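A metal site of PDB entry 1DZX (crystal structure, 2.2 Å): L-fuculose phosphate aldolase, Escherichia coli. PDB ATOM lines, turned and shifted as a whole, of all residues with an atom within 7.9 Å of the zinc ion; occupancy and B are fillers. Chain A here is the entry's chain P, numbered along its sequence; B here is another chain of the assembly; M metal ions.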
ATOM      1  N   ALA A  27      17.323  16.070 -14.118  1.00  0.00           N
ATOM      2  CA  ALA A  27      16.526  14.880 -13.838  1.00  0.00           C
ATOM      3  C   ALA A  27      15.351  14.966 -14.802  1.00  0.00           C
ATOM      4  O   ALA A  27      15.161  16.097 -15.309  1.00  0.00           O
ATOM      5  CB  ALA A  27      16.090  14.881 -12.400  1.00  0.00           C
ATOM      6  N   GLY A  28      14.580  13.915 -15.038  1.00  0.00           N
ATOM      7  CA  GLY A  28      13.422  14.135 -15.929  1.00  0.00           C
ATOM      8  C   GLY A  28      13.769  13.778 -17.377  1.00  0.00           C
ATOM      9  O   GLY A  28      14.873  13.921 -17.911  1.00  0.00           O
ATOM     10  N   ASN A  29      12.784  13.109 -17.971  1.00  0.00           N
ATOM     11  CA  ASN A  29      12.862  12.574 -19.325  1.00  0.00           C
ATOM     12  C   ASN A  29      11.431  12.481 -19.802  1.00  0.00           C
ATOM     13  O   ASN A  29      10.490  12.293 -19.031  1.00  0.00           O
ATOM     14  CB  ASN A  29      13.604  11.222 -19.386  1.00  0.00           C
ATOM     15  CG  ASN A  29      13.591  10.413 -18.107  1.00  0.00           C
ATOM     16  OD1 ASN A  29      12.655   9.689 -17.787  1.00  0.00           O
ATOM     17  ND2 ASN A  29      14.656  10.556 -17.327  1.00  0.00           N
ATOM     18  N   SER A  71      17.904   8.588 -22.855  1.00  0.00           N
ATOM     19  CA  SER A  71      17.855   8.762 -21.423  1.00  0.00           C
ATOM     20  C   SER A  71      18.282   7.505 -20.705  1.00  0.00           C
ATOM     21  O   SER A  71      17.939   6.386 -21.125  1.00  0.00           O
ATOM     22  CB  SER A  71      16.387   9.038 -21.023  1.00  0.00           C
ATOM     23  OG  SER A  71      16.188   8.735 -19.663  1.00  0.00           O
ATOM     24  N   SER A  72      18.905   7.621 -19.529  1.00  0.00           N
ATOM     25  CA  SER A  72      19.301   6.417 -18.808  1.00  0.00           C
ATOM     26  C   SER A  72      18.071   5.682 -18.306  1.00  0.00           C
ATOM     27  O   SER A  72      18.213   4.499 -17.994  1.00  0.00           O
ATOM     28  CB  SER A  72      20.228   6.775 -17.632  1.00  0.00           C
ATOM     29  OG  SER A  72      19.556   7.775 -16.838  1.00  0.00           O
ATOM     30  N   GLU A  73      16.897   6.320 -18.262  1.00  0.00           N
ATOM     31  CA  GLU A  73      15.681   5.695 -17.784  1.00  0.00           C
ATOM     32  C   GLU A  73      14.709   5.265 -18.869  1.00  0.00           C
ATOM     33  O   GLU A  73      13.501   5.123 -18.626  1.00  0.00           O
ATOM     34  CB  GLU A  73      14.957   6.660 -16.807  1.00  0.00           C
ATOM     35  CG  GLU A  73      15.954   7.345 -15.868  1.00  0.00           C
ATOM     36  CD  GLU A  73      15.355   7.893 -14.606  1.00  0.00           C
ATOM     37  OE1 GLU A  73      14.881   7.133 -13.719  1.00  0.00           O
ATOM     38  OE2 GLU A  73      15.342   9.139 -14.476  1.00  0.00           O
ATOM     39  N   PHE A  76      11.627   2.086 -18.617  1.00  0.00           N
ATOM     40  CA  PHE A  76      10.271   2.137 -18.040  1.00  0.00           C
ATOM     41  C   PHE A  76       9.377   2.994 -18.931  1.00  0.00           C
ATOM     42  O   PHE A  76       8.160   2.937 -18.754  1.00  0.00           O
ATOM     43  CB  PHE A  76      10.267   2.462 -16.578  1.00  0.00           C
ATOM     44  CG  PHE A  76      10.758   3.777 -16.071  1.00  0.00           C
ATOM     45  CD1 PHE A  76      10.599   4.960 -16.754  1.00  0.00           C
ATOM     46  CD2 PHE A  76      11.402   3.826 -14.838  1.00  0.00           C
ATOM     47  CE1 PHE A  76      11.079   6.153 -16.241  1.00  0.00           C
ATOM     48  CE2 PHE A  76      11.878   5.018 -14.302  1.00  0.00           C
ATOM     49  CZ  PHE A  76      11.713   6.180 -15.012  1.00  0.00           C
ATOM     50  N   HIS A  77       9.875   3.739 -19.906  1.00  0.00           N
ATOM     51  CA  HIS A  77       9.050   4.471 -20.851  1.00  0.00           C
ATOM     52  C   HIS A  77       8.481   3.412 -21.795  1.00  0.00           C
ATOM     53  O   HIS A  77       7.274   3.446 -22.096  1.00  0.00           O
ATOM     54  CB  HIS A  77       9.796   5.522 -21.666  1.00  0.00           C
ATOM     55  CG  HIS A  77      10.127   6.743 -20.875  1.00  0.00           C
ATOM     56  ND1 HIS A  77       9.438   7.925 -21.066  1.00  0.00           N
ATOM     57  CD2 HIS A  77      11.039   6.980 -19.908  1.00  0.00           C
ATOM     58  CE1 HIS A  77       9.920   8.860 -20.260  1.00  0.00           C
ATOM     59  NE2 HIS A  77      10.882   8.306 -19.527  1.00  0.00           N
ATOM     60  N   HIS A  92       8.334  11.859 -16.952  1.00  0.00           N
ATOM     61  CA  HIS A  92       8.902  11.379 -15.691  1.00  0.00           C
ATOM     62  C   HIS A  92       9.709  12.505 -15.070  1.00  0.00           C
ATOM     63  O   HIS A  92      10.502  13.150 -15.749  1.00  0.00           O
ATOM     64  CB  HIS A  92       9.790  10.154 -15.958  1.00  0.00           C
ATOM     65  CG  HIS A  92      10.647   9.780 -14.786  1.00  0.00           C
ATOM     66  ND1 HIS A  92      10.117   9.261 -13.628  1.00  0.00           N
ATOM     67  CD2 HIS A  92      12.001   9.828 -14.575  1.00  0.00           C
ATOM     68  CE1 HIS A  92      11.087   9.013 -12.762  1.00  0.00           C
ATOM     69  NE2 HIS A  92      12.235   9.339 -13.318  1.00  0.00           N
ATOM     70  N   ASN A  93       9.560  12.739 -13.772  1.00  0.00           N
ATOM     71  CA  ASN A  93      10.404  13.752 -13.131  1.00  0.00           C
ATOM     72  C   ASN A  93      10.641  13.258 -11.710  1.00  0.00           C
ATOM     73  O   ASN A  93      10.101  12.234 -11.271  1.00  0.00           O
ATOM     74  CB  ASN A  93       9.719  15.087 -13.167  1.00  0.00           C
ATOM     75  CG  ASN A  93       8.357  15.075 -12.487  1.00  0.00           C
ATOM     76  OD1 ASN A  93       8.223  14.656 -11.331  1.00  0.00           O
ATOM     77  ND2 ASN A  93       7.353  15.575 -13.214  1.00  0.00           N
ATOM     78  N   HIS A  94      11.461  13.972 -10.985  1.00  0.00           N
ATOM     79  CA  HIS A  94      11.742  13.776  -9.585  1.00  0.00           C
ATOM     80  C   HIS A  94      11.136  14.969  -8.827  1.00  0.00           C
ATOM     81  O   HIS A  94      11.793  15.566  -7.976  1.00  0.00           O
ATOM     82  CB  HIS A  94      13.246  13.632  -9.361  1.00  0.00           C
ATOM     83  CG  HIS A  94      13.915  12.492 -10.076  1.00  0.00           C
ATOM     84  ND1 HIS A  94      15.283  12.345 -10.008  1.00  0.00           N
ATOM     85  CD2 HIS A  94      13.482  11.484 -10.871  1.00  0.00           C
ATOM     86  CE1 HIS A  94      15.654  11.288 -10.758  1.00  0.00           C
ATOM     87  NE2 HIS A  94      14.570  10.751 -11.297  1.00  0.00           N
ATOM     88  N   PHE A 131      17.372   2.276 -10.787  1.00  0.00           N
ATOM     89  CA  PHE A 131      16.994   2.933 -12.036  1.00  0.00           C
ATOM     90  C   PHE A 131      17.571   2.114 -13.222  1.00  0.00           C
ATOM     91  O   PHE A 131      18.580   1.412 -13.072  1.00  0.00           O
ATOM     92  CB  PHE A 131      17.458   4.386 -12.149  1.00  0.00           C
ATOM     93  CG  PHE A 131      18.927   4.608 -12.383  1.00  0.00           C
ATOM     94  CD1 PHE A 131      19.825   4.488 -11.331  1.00  0.00           C
ATOM     95  CD2 PHE A 131      19.413   4.911 -13.635  1.00  0.00           C
ATOM     96  CE1 PHE A 131      21.183   4.662 -11.505  1.00  0.00           C
ATOM     97  CE2 PHE A 131      20.775   5.101 -13.835  1.00  0.00           C
ATOM     98  CZ  PHE A 131      21.651   4.975 -12.778  1.00  0.00           C
ATOM     99  N   GLY A 132      16.858   2.180 -14.347  1.00  0.00           N
ATOM    100  CA  GLY A 132      17.228   1.540 -15.574  1.00  0.00           C
ATOM    101  C   GLY A 132      17.180   0.028 -15.642  1.00  0.00           C
ATOM    102  O   GLY A 132      17.633  -0.545 -16.635  1.00  0.00           O
ATOM    103  N   LEU A 136      12.742  -2.619 -12.230  1.00  0.00           N
ATOM    104  CA  LEU A 136      11.982  -1.393 -12.060  1.00  0.00           C
ATOM    105  C   LEU A 136      10.814  -1.361 -13.069  1.00  0.00           C
ATOM    106  O   LEU A 136       9.672  -1.047 -12.793  1.00  0.00           O
ATOM    107  CB  LEU A 136      12.813  -0.116 -12.245  1.00  0.00           C
ATOM    108  CG  LEU A 136      12.569   1.088 -11.348  1.00  0.00           C
ATOM    109  CD1 LEU A 136      12.847   2.403 -12.041  1.00  0.00           C
ATOM    110  CD2 LEU A 136      11.203   1.119 -10.642  1.00  0.00           C
ATOM    111  N   LEU A 152       7.267   6.304  -7.549  1.00  0.00           N
ATOM    112  CA  LEU A 152       8.309   5.286  -7.589  1.00  0.00           C
ATOM    113  C   LEU A 152       9.046   5.444  -6.249  1.00  0.00           C
ATOM    114  O   LEU A 152       9.523   6.549  -6.017  1.00  0.00           O
ATOM    115  CB  LEU A 152       9.282   5.532  -8.723  1.00  0.00           C
ATOM    116  CG  LEU A 152       8.969   5.237 -10.172  1.00  0.00           C
ATOM    117  CD1 LEU A 152       7.883   4.185 -10.343  1.00  0.00           C
ATOM    118  CD2 LEU A 152       8.551   6.517 -10.887  1.00  0.00           C
ATOM    119  N   HIS A 154      11.446   6.087  -3.292  1.00  0.00           N
ATOM    120  CA  HIS A 154      12.779   6.661  -3.258  1.00  0.00           C
ATOM    121  C   HIS A 154      13.254   7.247  -4.574  1.00  0.00           C
ATOM    122  O   HIS A 154      14.445   7.189  -4.897  1.00  0.00           O
ATOM    123  CB  HIS A 154      13.850   5.612  -2.873  1.00  0.00           C
ATOM    124  CG  HIS A 154      13.758   5.268  -1.426  1.00  0.00           C
ATOM    125  ND1 HIS A 154      14.047   6.181  -0.441  1.00  0.00           N
ATOM    126  CD2 HIS A 154      13.390   4.114  -0.801  1.00  0.00           C
ATOM    127  CE1 HIS A 154      13.858   5.611   0.743  1.00  0.00           C
ATOM    128  NE2 HIS A 154      13.458   4.370   0.535  1.00  0.00           N
ATOM    129  N   HIS A 155      12.290   7.769  -5.352  1.00  0.00           N
ATOM    130  CA  HIS A 155      12.712   8.165  -6.712  1.00  0.00           C
ATOM    131  C   HIS A 155      11.934   9.306  -7.335  1.00  0.00           C
ATOM    132  O   HIS A 155      12.519  10.363  -7.626  1.00  0.00           O
ATOM    133  CB  HIS A 155      12.587   6.872  -7.524  1.00  0.00           C
ATOM    134  CG  HIS A 155      13.087   6.986  -8.927  1.00  0.00           C
ATOM    135  ND1 HIS A 155      13.662   5.904  -9.562  1.00  0.00           N
ATOM    136  CD2 HIS A 155      13.122   8.021  -9.800  1.00  0.00           C
ATOM    137  CE1 HIS A 155      14.039   6.286 -10.772  1.00  0.00           C
ATOM    138  NE2 HIS A 155      13.715   7.563 -10.961  1.00  0.00           N
ATOM    139  N   GLY A 156      10.657   9.088  -7.638  1.00  0.00           N
ATOM    140  CA  GLY A 156       9.908  10.149  -8.318  1.00  0.00           C
ATOM    141  C   GLY A 156       8.543   9.699  -8.816  1.00  0.00           C
ATOM    142  O   GLY A 156       7.783   8.989  -8.159  1.00  0.00           O
ATOM    143  N   LEU A 157       8.205  10.194 -10.004  1.00  0.00           N
ATOM    144  CA  LEU A 157       6.870  10.041 -10.562  1.00  0.00           C
ATOM    145  C   LEU A 157       6.897   9.718 -12.042  1.00  0.00           C
ATOM    146  O   LEU A 157       7.776  10.245 -12.744  1.00  0.00           O
ATOM    147  CB  LEU A 157       6.222  11.422 -10.395  1.00  0.00           C
ATOM    148  CG  LEU A 157       4.864  11.940 -10.766  1.00  0.00           C
ATOM    149  CD1 LEU A 157       4.805  12.341 -12.216  1.00  0.00           C
ATOM    150  CD2 LEU A 157       3.676  11.065 -10.452  1.00  0.00           C
ATOM    151  N   ILE A 158       5.911   8.957 -12.503  1.00  0.00           N
ATOM    152  CA  ILE A 158       5.664   8.719 -13.918  1.00  0.00           C
ATOM    153  C   ILE A 158       4.190   9.043 -14.202  1.00  0.00           C
ATOM    154  O   ILE A 158       3.277   8.604 -13.475  1.00  0.00           O
ATOM    155  CB  ILE A 158       5.853   7.237 -14.307  1.00  0.00           C
ATOM    156  CG1 ILE A 158       7.322   6.832 -14.239  1.00  0.00           C
ATOM    157  CG2 ILE A 158       5.250   6.903 -15.662  1.00  0.00           C
ATOM    158  CD1 ILE A 158       8.120   7.183 -15.481  1.00  0.00           C
ATOM    159  N   HIS B 112      17.205   9.121  -1.139  1.00  0.00           N
ATOM    160  CA  HIS B 112      16.998   9.135  -2.557  1.00  0.00           C
ATOM    161  C   HIS B 112      18.254   8.635  -3.262  1.00  0.00           C
ATOM    162  O   HIS B 112      19.376   8.906  -2.762  1.00  0.00           O
ATOM    163  CB  HIS B 112      16.764  10.564  -3.040  1.00  0.00           C
ATOM    164  CG  HIS B 112      16.174  10.626  -4.409  1.00  0.00           C
ATOM    165  ND1 HIS B 112      16.937  10.592  -5.562  1.00  0.00           N
ATOM    166  CD2 HIS B 112      14.886  10.701  -4.829  1.00  0.00           C
ATOM    167  CE1 HIS B 112      16.163  10.648  -6.621  1.00  0.00           C
ATOM    168  NE2 HIS B 112      14.908  10.720  -6.217  1.00  0.00           N
ATOM    169  N   TYR B 113      18.107   8.000  -4.431  1.00  0.00           N
ATOM    170  CA  TYR B 113      19.313   7.472  -5.079  1.00  0.00           C
ATOM    171  C   TYR B 113      20.235   8.552  -5.621  1.00  0.00           C
ATOM    172  O   TYR B 113      21.439   8.256  -5.780  1.00  0.00           O
ATOM    173  CB  TYR B 113      19.053   6.385  -6.119  1.00  0.00           C
ATOM    174  CG  TYR B 113      18.619   6.959  -7.453  1.00  0.00           C
ATOM    175  CD1 TYR B 113      17.246   7.113  -7.672  1.00  0.00           C
ATOM    176  CD2 TYR B 113      19.492   7.270  -8.481  1.00  0.00           C
ATOM    177  CE1 TYR B 113      16.764   7.618  -8.843  1.00  0.00           C
ATOM    178  CE2 TYR B 113      19.024   7.777  -9.672  1.00  0.00           C
ATOM    179  CZ  TYR B 113      17.664   7.956  -9.849  1.00  0.00           C
ATOM    180  OH  TYR B 113      17.141   8.455 -11.018  1.00  0.00           O
ATOM    181  N   MET B 114      19.804   9.789  -5.781  1.00  0.00           N
ATOM    182  CA  MET B 114      20.675  10.834  -6.257  1.00  0.00           C
ATOM    183  C   MET B 114      21.697  11.292  -5.229  1.00  0.00           C
ATOM    184  O   MET B 114      22.658  11.966  -5.636  1.00  0.00           O
ATOM    185  CB  MET B 114      19.915  12.050  -6.807  1.00  0.00           C
ATOM    186  CG  MET B 114      19.403  11.722  -8.215  1.00  0.00           C
ATOM    187  SD  MET B 114      20.670  11.817  -9.477  1.00  0.00           S
ATOM    188  CE  MET B 114      21.575  13.287  -9.018  1.00  0.00           C
HETATM  189 ZN    ZN M   1      14.219   9.080 -12.454  1.00  0.00          ZN
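The zinc ion is bound by a ring nitrogen (NE2) of His 94 (2.1 Å), a ring nitrogen (NE2) of His 92 (2.2 Å), a ring nitrogen (NE2) of His 155 (2.2 Å), the side-chain carboxylate (OE2) of Glu 73 (2.3 Å) and the side-chain carboxylate (OE1) of Glu 73 (2.4 Å).
Merely in contact with the zinc ion: Tyr 113 of chain B. Five residues have an atom within 4 Å of the zinc ion: Glu 73, His 92, His 94, His 155 and Tyr 113 of chain B.
The backbone carbonyl oxygen of Leu 157 lies within hydrogen-bond range of a ring nitrogen (ND1) of His 92 (2.7 Å). The side-chain hydroxyl (OH) of Tyr 113 of chain B lies close to a ring nitrogen (NE2) of His 94 (3.5 Å). The backbone NH of Glu 73 lies within hydrogen-bond range of the side-chain hydroxyl of Ser 71 (2.9 Å). OE2 of Glu 73 sits close to ND2 of Asn 29 (3.3 Å). A ring nitrogen (NE2) of His 112 of chain B is in hydrogen-bond range of the backbone carbonyl oxygen of His 155, 2.8 Å away. The backbone NH (N) of His 92 sits at hydrogen-bond distance from the backbone carbonyl oxygen (O) of Asn 29, 3.0 Å away.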
